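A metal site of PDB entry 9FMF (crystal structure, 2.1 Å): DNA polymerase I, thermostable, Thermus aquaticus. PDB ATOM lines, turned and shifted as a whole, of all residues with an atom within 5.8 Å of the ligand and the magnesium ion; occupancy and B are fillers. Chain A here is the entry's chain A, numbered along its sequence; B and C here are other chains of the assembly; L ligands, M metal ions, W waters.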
ATOM      1  N   ARG A 281       8.308   0.161  34.877  1.00  0.00           N
ATOM      2  CA  ARG A 281       7.588   1.280  35.452  1.00  0.00           C
ATOM      3  C   ARG A 281       7.256   1.020  36.925  1.00  0.00           C
ATOM      4  O   ARG A 281       7.153  -0.136  37.371  1.00  0.00           O
ATOM      5  CB  ARG A 281       6.301   1.550  34.686  1.00  0.00           C
ATOM      6  CG  ARG A 281       6.454   2.218  33.373  1.00  0.00           C
ATOM      7  CD  ARG A 281       5.063   2.608  32.924  1.00  0.00           C
ATOM      8  NE  ARG A 281       5.075   3.484  31.774  1.00  0.00           N
ATOM      9  CZ  ARG A 281       4.007   4.117  31.306  1.00  0.00           C
ATOM     10  NH1 ARG A 281       2.818   3.953  31.871  1.00  0.00           N
ATOM     11  NH2 ARG A 281       4.131   4.944  30.277  1.00  0.00           N
ATOM     12  N   VAL A 294      -7.712  14.297  34.274  1.00  0.00           N
ATOM     13  CA  VAL A 294      -7.165  15.575  33.826  1.00  0.00           C
ATOM     14  C   VAL A 294      -7.775  16.015  32.502  1.00  0.00           C
ATOM     15  O   VAL A 294      -7.849  17.217  32.216  1.00  0.00           O
ATOM     16  CB  VAL A 294      -5.643  15.491  33.748  1.00  0.00           C
ATOM     17  CG1 VAL A 294      -5.219  14.494  32.681  1.00  0.00           C
ATOM     18  CG2 VAL A 294      -5.051  16.873  33.487  1.00  0.00           C
ATOM     19  N   ARG A 295      -8.220  15.060  31.680  1.00  0.00           N
ATOM     20  CA  ARG A 295      -8.513  15.376  30.287  1.00  0.00           C
ATOM     21  C   ARG A 295      -9.831  16.115  30.116  1.00  0.00           C
ATOM     22  O   ARG A 295      -9.912  17.063  29.332  1.00  0.00           O
ATOM     23  CB  ARG A 295      -8.492  14.085  29.468  1.00  0.00           C
ATOM     24  CG  ARG A 295      -7.151  13.379  29.557  1.00  0.00           C
ATOM     25  CD  ARG A 295      -7.088  12.166  28.653  1.00  0.00           C
ATOM     26  NE  ARG A 295      -7.421  12.529  27.285  1.00  0.00           N
ATOM     27  CZ  ARG A 295      -7.294  11.733  26.242  1.00  0.00           C
ATOM     28  NH1 ARG A 295      -6.855  10.489  26.360  1.00  0.00           N
ATOM     29  NH2 ARG A 295      -7.591  12.205  25.023  1.00  0.00           N
ATOM     30  N   ASP A 318       7.748  17.268  33.687  1.00  0.00           N
ATOM     31  CA  ASP A 318       7.176  16.302  32.758  1.00  0.00           C
ATOM     32  C   ASP A 318       8.096  16.246  31.536  1.00  0.00           C
ATOM     33  O   ASP A 318       8.301  17.284  30.891  1.00  0.00           O
ATOM     34  CB  ASP A 318       5.747  16.750  32.362  1.00  0.00           C
ATOM     35  CG  ASP A 318       4.965  15.704  31.487  1.00  0.00           C
ATOM     36  OD1 ASP A 318       5.576  14.852  30.793  1.00  0.00           O
ATOM     37  OD2 ASP A 318       3.698  15.759  31.490  1.00  0.00           O
ATOM     38  N   TYR A 319       8.680  15.081  31.253  1.00  0.00           N
ATOM     39  CA  TYR A 319       9.483  14.893  30.051  1.00  0.00           C
ATOM     40  C   TYR A 319       8.609  15.027  28.807  1.00  0.00           C
ATOM     41  O   TYR A 319       7.504  14.469  28.749  1.00  0.00           O
ATOM     42  CB  TYR A 319      10.155  13.521  30.032  1.00  0.00           C
ATOM     43  CG  TYR A 319      11.331  13.373  30.958  1.00  0.00           C
ATOM     44  CD1 TYR A 319      12.513  14.049  30.721  1.00  0.00           C
ATOM     45  CD2 TYR A 319      11.260  12.532  32.062  1.00  0.00           C
ATOM     46  CE1 TYR A 319      13.617  13.915  31.581  1.00  0.00           C
ATOM     47  CE2 TYR A 319      12.346  12.383  32.926  1.00  0.00           C
ATOM     48  CZ  TYR A 319      13.515  13.068  32.673  1.00  0.00           C
ATOM     49  OH  TYR A 319      14.580  12.910  33.536  1.00  0.00           O
ATOM     50  N   SER A 320       9.133  15.723  27.795  1.00  0.00           N
ATOM     51  CA  SER A 320       8.390  15.904  26.554  1.00  0.00           C
ATOM     52  C   SER A 320       8.662  14.762  25.585  1.00  0.00           C
ATOM     53  O   SER A 320       9.817  14.376  25.391  1.00  0.00           O
ATOM     54  CB  SER A 320       8.771  17.218  25.877  1.00  0.00           C
ATOM     55  OG  SER A 320       9.657  16.955  24.810  1.00  0.00           O
ATOM     56  N   GLN A 321       7.593  14.241  24.959  1.00  0.00           N
ATOM     57  CA  GLN A 321       7.691  13.234  23.900  1.00  0.00           C
ATOM     58  C   GLN A 321       8.712  12.155  24.254  1.00  0.00           C
ATOM     59  O   GLN A 321       9.593  11.810  23.478  1.00  0.00           O
ATOM     60  CB  GLN A 321       8.036  13.864  22.560  1.00  0.00           C
ATOM     61  CG  GLN A 321       7.250  15.119  22.192  1.00  0.00           C
ATOM     62  CD  GLN A 321       7.718  15.750  20.884  1.00  0.00           C
ATOM     63  OE1 GLN A 321       7.431  15.244  19.793  1.00  0.00           O
ATOM     64  NE2 GLN A 321       8.442  16.866  20.992  1.00  0.00           N
ATOM     65  N   ILE A 322       8.580  11.631  25.472  1.00  0.00           N
ATOM     66  CA  ILE A 322       9.694  10.928  26.080  1.00  0.00           C
ATOM     67  C   ILE A 322       9.994   9.623  25.339  1.00  0.00           C
ATOM     68  O   ILE A 322      11.130   9.359  24.960  1.00  0.00           O
ATOM     69  CB  ILE A 322       9.447  10.712  27.587  1.00  0.00           C
ATOM     70  CG1 ILE A 322      10.547   9.840  28.190  1.00  0.00           C
ATOM     71  CG2 ILE A 322       8.060  10.167  27.839  1.00  0.00           C
ATOM     72  CD1 ILE A 322      11.871  10.590  28.405  1.00  0.00           C
ATOM     73  N   GLU A 323       8.964   8.801  25.095  1.00  0.00           N
ATOM     74  CA  GLU A 323       9.230   7.518  24.428  1.00  0.00           C
ATOM     75  C   GLU A 323       9.634   7.682  22.970  1.00  0.00           C
ATOM     76  O   GLU A 323      10.259   6.770  22.409  1.00  0.00           O
ATOM     77  CB  GLU A 323       8.015   6.584  24.577  1.00  0.00           C
ATOM     78  CG  GLU A 323       7.842   6.097  26.052  1.00  0.00           C
ATOM     79  CD  GLU A 323       6.699   5.099  26.289  1.00  0.00           C
ATOM     80  OE1 GLU A 323       6.295   4.363  25.357  1.00  0.00           O
ATOM     81  OE2 GLU A 323       6.193   5.067  27.446  1.00  0.00           O
ATOM     82  N   LEU A 324       9.366   8.835  22.333  1.00  0.00           N
ATOM     83  CA  LEU A 324       9.854   9.046  20.980  1.00  0.00           C
ATOM     84  C   LEU A 324      11.346   9.381  20.967  1.00  0.00           C
ATOM     85  O   LEU A 324      12.085   8.890  20.105  1.00  0.00           O
ATOM     86  CB  LEU A 324       9.050  10.151  20.277  1.00  0.00           C
ATOM     87  CG  LEU A 324       7.571   9.847  20.033  1.00  0.00           C
ATOM     88  CD1 LEU A 324       6.796  11.069  19.572  1.00  0.00           C
ATOM     89  CD2 LEU A 324       7.464   8.746  18.993  1.00  0.00           C
ATOM     90  N   HIS A 347       3.605  15.401  18.298  1.00  0.00           N
ATOM     91  CA  HIS A 347       2.190  15.379  18.656  1.00  0.00           C
ATOM     92  C   HIS A 347       1.438  16.587  18.105  1.00  0.00           C
ATOM     93  O   HIS A 347       0.282  16.447  17.715  1.00  0.00           O
ATOM     94  CB  HIS A 347       2.010  15.294  20.181  1.00  0.00           C
ATOM     95  CG  HIS A 347       2.744  14.151  20.817  1.00  0.00           C
ATOM     96  ND1 HIS A 347       2.989  12.961  20.175  1.00  0.00           N
ATOM     97  CD2 HIS A 347       3.301  14.024  22.054  1.00  0.00           C
ATOM     98  CE1 HIS A 347       3.648  12.147  20.980  1.00  0.00           C
ATOM     99  NE2 HIS A 347       3.858  12.772  22.131  1.00  0.00           N
ATOM    100  N   ARG A 367      -4.010  18.193  20.751  1.00  0.00           N
ATOM    101  CA  ARG A 367      -2.719  17.542  20.942  1.00  0.00           C
ATOM    102  C   ARG A 367      -2.873  16.233  21.711  1.00  0.00           C
ATOM    103  O   ARG A 367      -2.217  15.243  21.399  1.00  0.00           O
ATOM    104  CB  ARG A 367      -1.765  18.492  21.663  1.00  0.00           C
ATOM    105  CG  ARG A 367      -0.285  18.169  21.510  1.00  0.00           C
ATOM    106  CD  ARG A 367       0.607  19.156  22.284  1.00  0.00           C
ATOM    107  NE  ARG A 367       1.990  18.704  22.306  1.00  0.00           N
ATOM    108  CZ  ARG A 367       2.487  17.876  23.209  1.00  0.00           C
ATOM    109  NH1 ARG A 367       1.766  17.468  24.243  1.00  0.00           N
ATOM    110  NH2 ARG A 367       3.736  17.438  23.075  1.00  0.00           N
ATOM    111  N   ARG A 368      -3.763  16.223  22.711  1.00  0.00           N
ATOM    112  CA  ARG A 368      -4.024  15.001  23.466  1.00  0.00           C
ATOM    113  C   ARG A 368      -4.508  13.887  22.548  1.00  0.00           C
ATOM    114  O   ARG A 368      -4.153  12.717  22.726  1.00  0.00           O
ATOM    115  CB  ARG A 368      -5.048  15.263  24.573  1.00  0.00           C
ATOM    116  CG  ARG A 368      -4.610  16.246  25.658  1.00  0.00           C
ATOM    117  CD  ARG A 368      -5.720  16.399  26.702  1.00  0.00           C
ATOM    118  NE  ARG A 368      -5.510  17.490  27.655  1.00  0.00           N
ATOM    119  CZ  ARG A 368      -4.624  17.472  28.645  1.00  0.00           C
ATOM    120  NH1 ARG A 368      -3.754  16.496  28.796  1.00  0.00           N
ATOM    121  NH2 ARG A 368      -4.600  18.491  29.507  1.00  0.00           N
ATOM    122  N   ALA A 369      -5.336  14.226  21.564  1.00  0.00           N
ATOM    123  CA  ALA A 369      -5.833  13.213  20.645  1.00  0.00           C
ATOM    124  C   ALA A 369      -4.707  12.653  19.785  1.00  0.00           C
ATOM    125  O   ALA A 369      -4.627  11.444  19.541  1.00  0.00           O
ATOM    126  CB  ALA A 369      -6.937  13.804  19.770  1.00  0.00           C
ATOM    127  N   LYS A 371      -1.614  12.471  20.645  1.00  0.00           N
ATOM    128  CA  LYS A 371      -0.730  11.636  21.462  1.00  0.00           C
ATOM    129  C   LYS A 371      -1.180  10.183  21.418  1.00  0.00           C
ATOM    130  O   LYS A 371      -0.401   9.281  21.112  1.00  0.00           O
ATOM    131  CB  LYS A 371      -0.689  12.157  22.898  1.00  0.00           C
ATOM    132  CG  LYS A 371       0.200  13.367  23.052  1.00  0.00           C
ATOM    133  CD  LYS A 371      -0.097  14.156  24.317  1.00  0.00           C
ATOM    134  CE  LYS A 371       0.236  13.369  25.532  1.00  0.00           C
ATOM    135  NZ  LYS A 371       1.650  13.621  25.886  1.00  0.00           N
ATOM    136  N   THR A 372      -2.472   9.935  21.695  1.00  0.00           N
ATOM    137  CA  THR A 372      -2.950   8.560  21.660  1.00  0.00           C
ATOM    138  C   THR A 372      -2.856   7.976  20.255  1.00  0.00           C
ATOM    139  O   THR A 372      -2.580   6.783  20.096  1.00  0.00           O
ATOM    140  CB  THR A 372      -4.384   8.503  22.196  1.00  0.00           C
ATOM    141  OG1 THR A 372      -5.313   8.527  21.100  1.00  0.00           O
ATOM    142  CG2 THR A 372      -4.660   9.663  23.122  1.00  0.00           C
ATOM    143  N   PHE A 375       1.068   7.172  19.540  1.00  0.00           N
ATOM    144  CA  PHE A 375       1.505   6.001  20.280  1.00  0.00           C
ATOM    145  C   PHE A 375       0.693   4.776  19.898  1.00  0.00           C
ATOM    146  O   PHE A 375       1.218   3.657  19.937  1.00  0.00           O
ATOM    147  CB  PHE A 375       1.441   6.289  21.785  1.00  0.00           C
ATOM    148  CG  PHE A 375       2.493   7.279  22.240  1.00  0.00           C
ATOM    149  CD1 PHE A 375       3.833   7.087  21.896  1.00  0.00           C
ATOM    150  CD2 PHE A 375       2.146   8.434  22.932  1.00  0.00           C
ATOM    151  CE1 PHE A 375       4.807   7.977  22.261  1.00  0.00           C
ATOM    152  CE2 PHE A 375       3.135   9.356  23.297  1.00  0.00           C
ATOM    153  CZ  PHE A 375       4.458   9.111  22.962  1.00  0.00           C
ATOM    154  N   GLY A 376      -0.551   4.964  19.485  1.00  0.00           N
ATOM    155  CA  GLY A 376      -1.299   3.857  18.927  1.00  0.00           C
ATOM    156  C   GLY A 376      -0.642   3.284  17.693  1.00  0.00           C
ATOM    157  O   GLY A 376      -0.393   2.081  17.615  1.00  0.00           O
ATOM    158  N   TYR A 379       2.998   1.483  18.273  1.00  0.00           N
ATOM    159  CA  TYR A 379       3.080   0.171  18.892  1.00  0.00           C
ATOM    160  C   TYR A 379       2.251  -0.878  18.195  1.00  0.00           C
ATOM    161  O   TYR A 379       2.083  -1.965  18.751  1.00  0.00           O
ATOM    162  CB  TYR A 379       2.681   0.264  20.365  1.00  0.00           C
ATOM    163  CG  TYR A 379       3.698   1.042  21.127  1.00  0.00           C
ATOM    164  CD1 TYR A 379       5.019   0.620  21.162  1.00  0.00           C
ATOM    165  CD2 TYR A 379       3.352   2.199  21.789  1.00  0.00           C
ATOM    166  CE1 TYR A 379       5.972   1.346  21.840  1.00  0.00           C
ATOM    167  CE2 TYR A 379       4.287   2.919  22.483  1.00  0.00           C
ATOM    168  CZ  TYR A 379       5.601   2.482  22.503  1.00  0.00           C
ATOM    169  OH  TYR A 379       6.526   3.212  23.197  1.00  0.00           O
ATOM    170  N   ASN A 458       7.688  -3.118  22.671  1.00  0.00           N
ATOM    171  CA  ASN A 458       7.317  -1.960  23.472  1.00  0.00           C
ATOM    172  C   ASN A 458       8.169  -1.852  24.726  1.00  0.00           C
ATOM    173  O   ASN A 458       8.514  -0.751  25.151  1.00  0.00           O
ATOM    174  CB  ASN A 458       5.851  -2.029  23.861  1.00  0.00           C
ATOM    175  CG  ASN A 458       5.518  -1.086  24.971  1.00  0.00           C
ATOM    176  OD1 ASN A 458       5.432  -1.484  26.129  1.00  0.00           O
ATOM    177  ND2 ASN A 458       5.357   0.183  24.640  1.00  0.00           N
ATOM    178  N   GLN A 462       9.582   1.611  26.587  1.00  0.00           N
ATOM    179  CA  GLN A 462       8.880   2.129  27.757  1.00  0.00           C
ATOM    180  C   GLN A 462       9.684   1.887  29.029  1.00  0.00           C
ATOM    181  O   GLN A 462       9.627   2.702  29.954  1.00  0.00           O
ATOM    182  CB  GLN A 462       7.487   1.502  27.847  1.00  0.00           C
ATOM    183  CG  GLN A 462       6.766   1.812  29.147  1.00  0.00           C
ATOM    184  CD  GLN A 462       5.539   0.929  29.364  1.00  0.00           C
ATOM    185  OE1 GLN A 462       5.457   0.178  30.337  1.00  0.00           O
ATOM    186  NE2 GLN A 462       4.563   1.044  28.461  1.00  0.00           N
ATOM    187  N   ASP A 493       6.419   9.643  33.673  1.00  0.00           N
ATOM    188  CA  ASP A 493       7.416  10.522  33.077  1.00  0.00           C
ATOM    189  C   ASP A 493       7.395  11.895  33.735  1.00  0.00           C
ATOM    190  O   ASP A 493       8.002  12.835  33.227  1.00  0.00           O
ATOM    191  CB  ASP A 493       7.236  10.623  31.557  1.00  0.00           C
ATOM    192  CG  ASP A 493       6.068  11.502  31.153  1.00  0.00           C
ATOM    193  OD1 ASP A 493       4.996  11.426  31.807  1.00  0.00           O
ATOM    194  OD2 ASP A 493       6.219  12.276  30.177  1.00  0.00           O
ATOM    195  P    DA B   4      -5.385  -3.092  17.491  1.00  0.00           P
ATOM    196  OP1  DA B   4      -6.538  -2.837  18.368  1.00  0.00           O
ATOM    197  OP2  DA B   4      -5.477  -2.760  16.052  1.00  0.00           O
ATOM    198  O5'  DA B   4      -4.132  -2.319  18.104  1.00  0.00           O
ATOM    199  C5'  DA B   4      -3.686  -2.639  19.413  1.00  0.00           C
ATOM    200  C4'  DA B   4      -2.222  -2.306  19.569  1.00  0.00           C
ATOM    201  O4'  DA B   4      -2.011  -0.913  19.235  1.00  0.00           O
ATOM    202  C3'  DA B   4      -1.687  -2.460  20.977  1.00  0.00           C
ATOM    203  O3'  DA B   4      -1.216  -3.782  21.150  1.00  0.00           O
ATOM    204  C2'  DA B   4      -0.547  -1.450  21.015  1.00  0.00           C
ATOM    205  C1'  DA B   4      -1.102  -0.319  20.145  1.00  0.00           C
ATOM    206  N9   DA B   4      -1.812   0.736  20.865  1.00  0.00           N
ATOM    207  C8   DA B   4      -3.148   1.064  20.771  1.00  0.00           C
ATOM    208  N7   DA B   4      -3.513   2.070  21.533  1.00  0.00           N
ATOM    209  C5   DA B   4      -2.343   2.424  22.177  1.00  0.00           C
ATOM    210  C6   DA B   4      -2.051   3.438  23.100  1.00  0.00           C
ATOM    211  N6   DA B   4      -2.968   4.289  23.563  1.00  0.00           N
ATOM    212  N1   DA B   4      -0.769   3.543  23.543  1.00  0.00           N
ATOM    213  C2   DA B   4       0.147   2.692  23.081  1.00  0.00           C
ATOM    214  N3   DA B   4      -0.001   1.697  22.202  1.00  0.00           N
ATOM    215  C4   DA B   4      -1.285   1.617  21.775  1.00  0.00           C
ATOM    216  P    DG B   5      -1.520  -4.565  22.516  1.00  0.00           P
ATOM    217  OP1  DG B   5      -1.222  -5.998  22.271  1.00  0.00           O
ATOM    218  OP2  DG B   5      -2.869  -4.181  23.013  1.00  0.00           O
ATOM    219  O5'  DG B   5      -0.478  -3.956  23.567  1.00  0.00           O
ATOM    220  C5'  DG B   5       0.907  -4.136  23.398  1.00  0.00           C
ATOM    221  C4'  DG B   5       1.702  -3.201  24.311  1.00  0.00           C
ATOM    222  O4'  DG B   5       1.408  -1.824  24.003  1.00  0.00           O
ATOM    223  C3'  DG B   5       1.408  -3.307  25.792  1.00  0.00           C
ATOM    224  O3'  DG B   5       2.110  -4.420  26.366  1.00  0.00           O
ATOM    225  C2'  DG B   5       1.965  -1.980  26.289  1.00  0.00           C
ATOM    226  C1'  DG B   5       1.617  -1.032  25.162  1.00  0.00           C
ATOM    227  N9   DG B   5       0.406  -0.295  25.413  1.00  0.00           N
ATOM    228  C8   DG B   5      -0.827  -0.541  24.894  1.00  0.00           C
ATOM    229  N7   DG B   5      -1.747   0.290  25.317  1.00  0.00           N
ATOM    230  C5   DG B   5      -1.055   1.149  26.149  1.00  0.00           C
ATOM    231  C6   DG B   5      -1.516   2.289  26.885  1.00  0.00           C
ATOM    232  O6   DG B   5      -2.667   2.750  26.942  1.00  0.00           O
ATOM    233  N1   DG B   5      -0.494   2.866  27.631  1.00  0.00           N
ATOM    234  C2   DG B   5       0.802   2.441  27.641  1.00  0.00           C
ATOM    235  N2   DG B   5       1.645   3.143  28.416  1.00  0.00           N
ATOM    236  N3   DG B   5       1.255   1.407  26.937  1.00  0.00           N
ATOM    237  C4   DG B   5       0.260   0.804  26.230  1.00  0.00           C
ATOM    238  P    DA C  11      -8.073  10.734  32.186  1.00  0.00           P
ATOM    239  OP1  DA C  11      -8.092  12.193  32.430  1.00  0.00           O
ATOM    240  OP2  DA C  11      -8.401  10.183  30.865  1.00  0.00           O
ATOM    241  O5'  DA C  11      -6.596  10.253  32.571  1.00  0.00           O
ATOM    242  C5'  DA C  11      -6.141  10.531  33.868  1.00  0.00           C
ATOM    243  C4'  DA C  11      -4.849   9.819  34.165  1.00  0.00           C
ATOM    244  O4'  DA C  11      -5.059   8.394  34.184  1.00  0.00           O
ATOM    245  C3'  DA C  11      -3.735  10.087  33.174  1.00  0.00           C
ATOM    246  O3'  DA C  11      -2.921  11.150  33.684  1.00  0.00           O
ATOM    247  C2'  DA C  11      -2.945   8.780  33.152  1.00  0.00           C
ATOM    248  C1'  DA C  11      -3.929   7.728  33.681  1.00  0.00           C
ATOM    249  N9   DA C  11      -4.349   6.786  32.654  1.00  0.00           N
ATOM    250  C8   DA C  11      -5.381   6.918  31.747  1.00  0.00           C
ATOM    251  N7   DA C  11      -5.480   5.899  30.915  1.00  0.00           N
ATOM    252  C5   DA C  11      -4.463   5.047  31.318  1.00  0.00           C
ATOM    253  C6   DA C  11      -4.028   3.780  30.875  1.00  0.00           C
ATOM    254  N6   DA C  11      -4.603   3.133  29.862  1.00  0.00           N
ATOM    255  N1   DA C  11      -2.979   3.208  31.504  1.00  0.00           N
ATOM    256  C2   DA C  11      -2.401   3.856  32.534  1.00  0.00           C
ATOM    257  N3   DA C  11      -2.708   5.045  33.039  1.00  0.00           N
ATOM    258  C4   DA C  11      -3.762   5.586  32.391  1.00  0.00           C
ATOM    259  N1  DOC C  12      -0.271   6.938  30.486  1.00  0.00           N
ATOM    260  C2  DOC C  12      -0.074   5.721  29.748  1.00  0.00           C
ATOM    261  N3  DOC C  12      -1.072   5.321  28.835  1.00  0.00           N
ATOM    262  C4  DOC C  12      -2.187   6.075  28.710  1.00  0.00           C
ATOM    263  C5  DOC C  12      -2.393   7.303  29.449  1.00  0.00           C
ATOM    264  C6  DOC C  12      -1.415   7.679  30.309  1.00  0.00           C
ATOM    265  O2  DOC C  12       0.948   5.090  29.929  1.00  0.00           O
ATOM    266  N4  DOC C  12      -3.134   5.625  27.828  1.00  0.00           N
ATOM    267  C1' DOC C  12       0.747   7.437  31.446  1.00  0.00           C
ATOM    268  C2' DOC C  12       1.906   8.181  30.719  1.00  0.00           C
ATOM    269  C3' DOC C  12       1.615   9.644  31.031  1.00  0.00           C
ATOM    270  C4' DOC C  12       1.031   9.507  32.416  1.00  0.00           C
ATOM    271  O4' DOC C  12       0.182   8.348  32.338  1.00  0.00           O
ATOM    272  C5' DOC C  12       0.136  10.651  32.817  1.00  0.00           C
ATOM    273  O5' DOC C  12      -0.902  10.778  31.906  1.00  0.00           O
ATOM    274  P   DOC C  12      -2.196  11.641  32.359  1.00  0.00           P
ATOM    275  OP1 DOC C  12      -1.758  12.866  33.056  1.00  0.00           O
ATOM    276  OP2 DOC C  12      -3.092  11.906  31.088  1.00  0.00           O
HETATM  277  C1  LIG L   1       4.549   8.401  27.765  1.00  0.00           C
HETATM  278  C2  LIG L   1       4.351   9.671  28.550  1.00  0.00           C
HETATM  279  C3  LIG L   1      -0.670   6.717  25.318  1.00  0.00           C
HETATM  280  C4  LIG L   1       1.109   7.746  26.590  1.00  0.00           C
HETATM  281  C5  LIG L   1      -0.158   7.835  26.067  1.00  0.00           C
HETATM  282  C6  LIG L   1      -0.977   9.035  26.262  1.00  0.00           C
HETATM  283  C7  LIG L   1      -2.012   9.538  25.561  1.00  0.00           C
HETATM  284  C8  LIG L   1      -2.455  10.713  26.267  1.00  0.00           C
HETATM  285  C9  LIG L   1      -3.497  11.641  26.161  1.00  0.00           C
HETATM  286  C10 LIG L   1      -3.641  12.584  27.145  1.00  0.00           C
HETATM  287  C11 LIG L   1      -2.810  12.682  28.233  1.00  0.00           C
HETATM  288  C12 LIG L   1      -1.770  11.780  28.355  1.00  0.00           C
HETATM  289  C13 LIG L   1      -1.617  10.826  27.370  1.00  0.00           C
HETATM  290  C14 LIG L   1       1.482   5.548  25.683  1.00  0.00           C
HETATM  291  C15 LIG L   1       3.328   6.631  26.861  1.00  0.00           C
HETATM  292  C16 LIG L   1       4.309   7.143  25.798  1.00  0.00           C
HETATM  293  C17 LIG L   1       4.591   8.572  26.254  1.00  0.00           C
HETATM  294  F1  LIG L   1      -4.689  13.450  27.064  1.00  0.00           F
HETATM  295  N1  LIG L   1       0.208   5.649  25.177  1.00  0.00           N
HETATM  296  N2  LIG L   1       1.916   6.648  26.392  1.00  0.00           N
HETATM  297  O1  LIG L   1      -1.788   6.662  24.820  1.00  0.00           O
HETATM  298  O2  LIG L   1       5.854   9.048  25.777  1.00  0.00           O
HETATM  299  O3  LIG L   1       3.027  10.166  28.297  1.00  0.00           O
HETATM  300  O4  LIG L   1       3.744  12.405  29.050  1.00  0.00           O
HETATM  301  O5  LIG L   1       1.386  12.091  28.181  1.00  0.00           O
HETATM  302  O6  LIG L   1       3.367  11.816  26.618  1.00  0.00           O
HETATM  303  O7  LIG L   1       5.708  12.555  27.067  1.00  0.00           O
HETATM  304  O8  LIG L   1       5.088  11.704  24.759  1.00  0.00           O
HETATM  305  O9  LIG L   1       4.095  13.873  25.641  1.00  0.00           O
HETATM  306  O10 LIG L   1       5.154  16.005  25.396  1.00  0.00           O
HETATM  307  O11 LIG L   1       2.751  16.082  26.166  1.00  0.00           O
HETATM  308  O12 LIG L   1       4.539  15.181  27.699  1.00  0.00           O
HETATM  309  O13 LIG L   1       3.444   7.493  27.981  1.00  0.00           O
HETATM  310  O14 LIG L   1      -0.705   9.799  27.378  1.00  0.00           O
HETATM  311  O15 LIG L   1       2.184   4.566  25.474  1.00  0.00           O
HETATM  312  P1  LIG L   1       2.819  11.723  28.122  1.00  0.00           P
HETATM  313  P2  LIG L   1       4.700  12.435  25.992  1.00  0.00           P
HETATM  314  P3  LIG L   1       4.085  15.379  26.261  1.00  0.00           P
HETATM  315 MG    MG M   1       5.649  13.734  28.802  1.00  0.00          MG
HETATM  316  O   HOH W   1       3.032  12.948  32.148  1.00  0.00           O
HETATM  317  O   HOH W   2       2.428  15.889  28.995  1.00  0.00           O
HETATM  318  O   HOH W   3       1.182  13.500  30.318  1.00  0.00           O
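Water W2 lies within hydrogen-bond range of OD2 of Asp 318 (2.8 Å) and O11 of the ligand (2.9 Å). Water W1 lies within hydrogen-bond range of OD1 of Asp 493 and OD2 of Asp 318.
OP1 of DA 11 of chain C sits at hydrogen-bond distance from the backbone NH (N) of Arg 295 (3.0 Å). N2 of DG 5 of chain B sits close to O2 of DOC 12 of chain C, at 2.6 Å. O2 of DOC 12 of chain C is in hydrogen-bond range of NH1 of Arg 281 (2.9 Å). The side-chain carboxylate of Glu 323 is in salt-bridge range of the guanidinium group of Arg 281 (3.5 Å). The side-chain hydroxyl (OH) of Tyr 379 is in hydrogen-bond range of the side-chain carboxylate (OE1) of Glu 323 (2.5 Å). The side-chain hydroxyl of Thr 372 lies within hydrogen-bond range of the backbone carbonyl oxygen of Ala 369.
A fluorine (F1) of the ligand sits close to the guanidinium group (NE) of Arg 295 (2.9 Å). An oxygen (O15) of the ligand sits close to N2 of DG 5 of chain B (3.3 Å). N4 of DOC 12 of chain C sits close to an oxygen (O1) of the ligand (3.5 Å). Ser 320 touches the ligand. CB of Arg 368 touches F1 of the ligand, 3.1 Å away. Thr 372 touches the ligand (CG2 to C7, 3.6 Å). CZ of Phe 375 touches O2 of the ligand, at 3.1 Å. Of the 26 residues printed, 18 come within 4 Å of the ligand.
Within 4 Å of the magnesium ion: Asp 318, Tyr 319 and Asp 493. Along chain A the residues within 4 Å of the magnesium ion span positions 318 to 493. The nearest printed residue that does not touch the magnesium ion is Ser 320 (4.1 Å).
The side-chain amino group of Lys 371 lies within salt-bridge range of an oxygen (O11) of the ligand (2.7 Å). The guanidinium group (NH1) of Arg 367 is in salt-bridge range of an oxygen (O11) of the ligand (2.6 Å). N1 of DA 4 of chain B sits at hydrogen-bond distance from a nitrogen (N1) of the ligand (2.8 Å). The backbone NH (N) of Gln 321 sits at hydrogen-bond distance from an oxygen (O10) of the ligand (3.0 Å). A ring nitrogen (NE2) of His 347 is in hydrogen-bond range of an oxygen (O8) of the ligand, 3.1 Å away. The backbone NH of Glu 323 lies within hydrogen-bond range of an oxygen (O2) of the ligand. N of Ile 322 sits close to O7 of the ligand. An oxygen (O13) of the ligand sits at hydrogen-bond distance from the guanidinium group of Arg 281 (3.5 Å).
The magnesium ion is bound by O of Tyr 319 (2.0 Å), OD2 of Asp 493 (2.1 Å), O7 of the ligand (2.1 Å), O12 of the ligand (2.1 Å), OD1 of Asp 318 (2.3 Å) and O4 of the ligand (2.3 Å).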
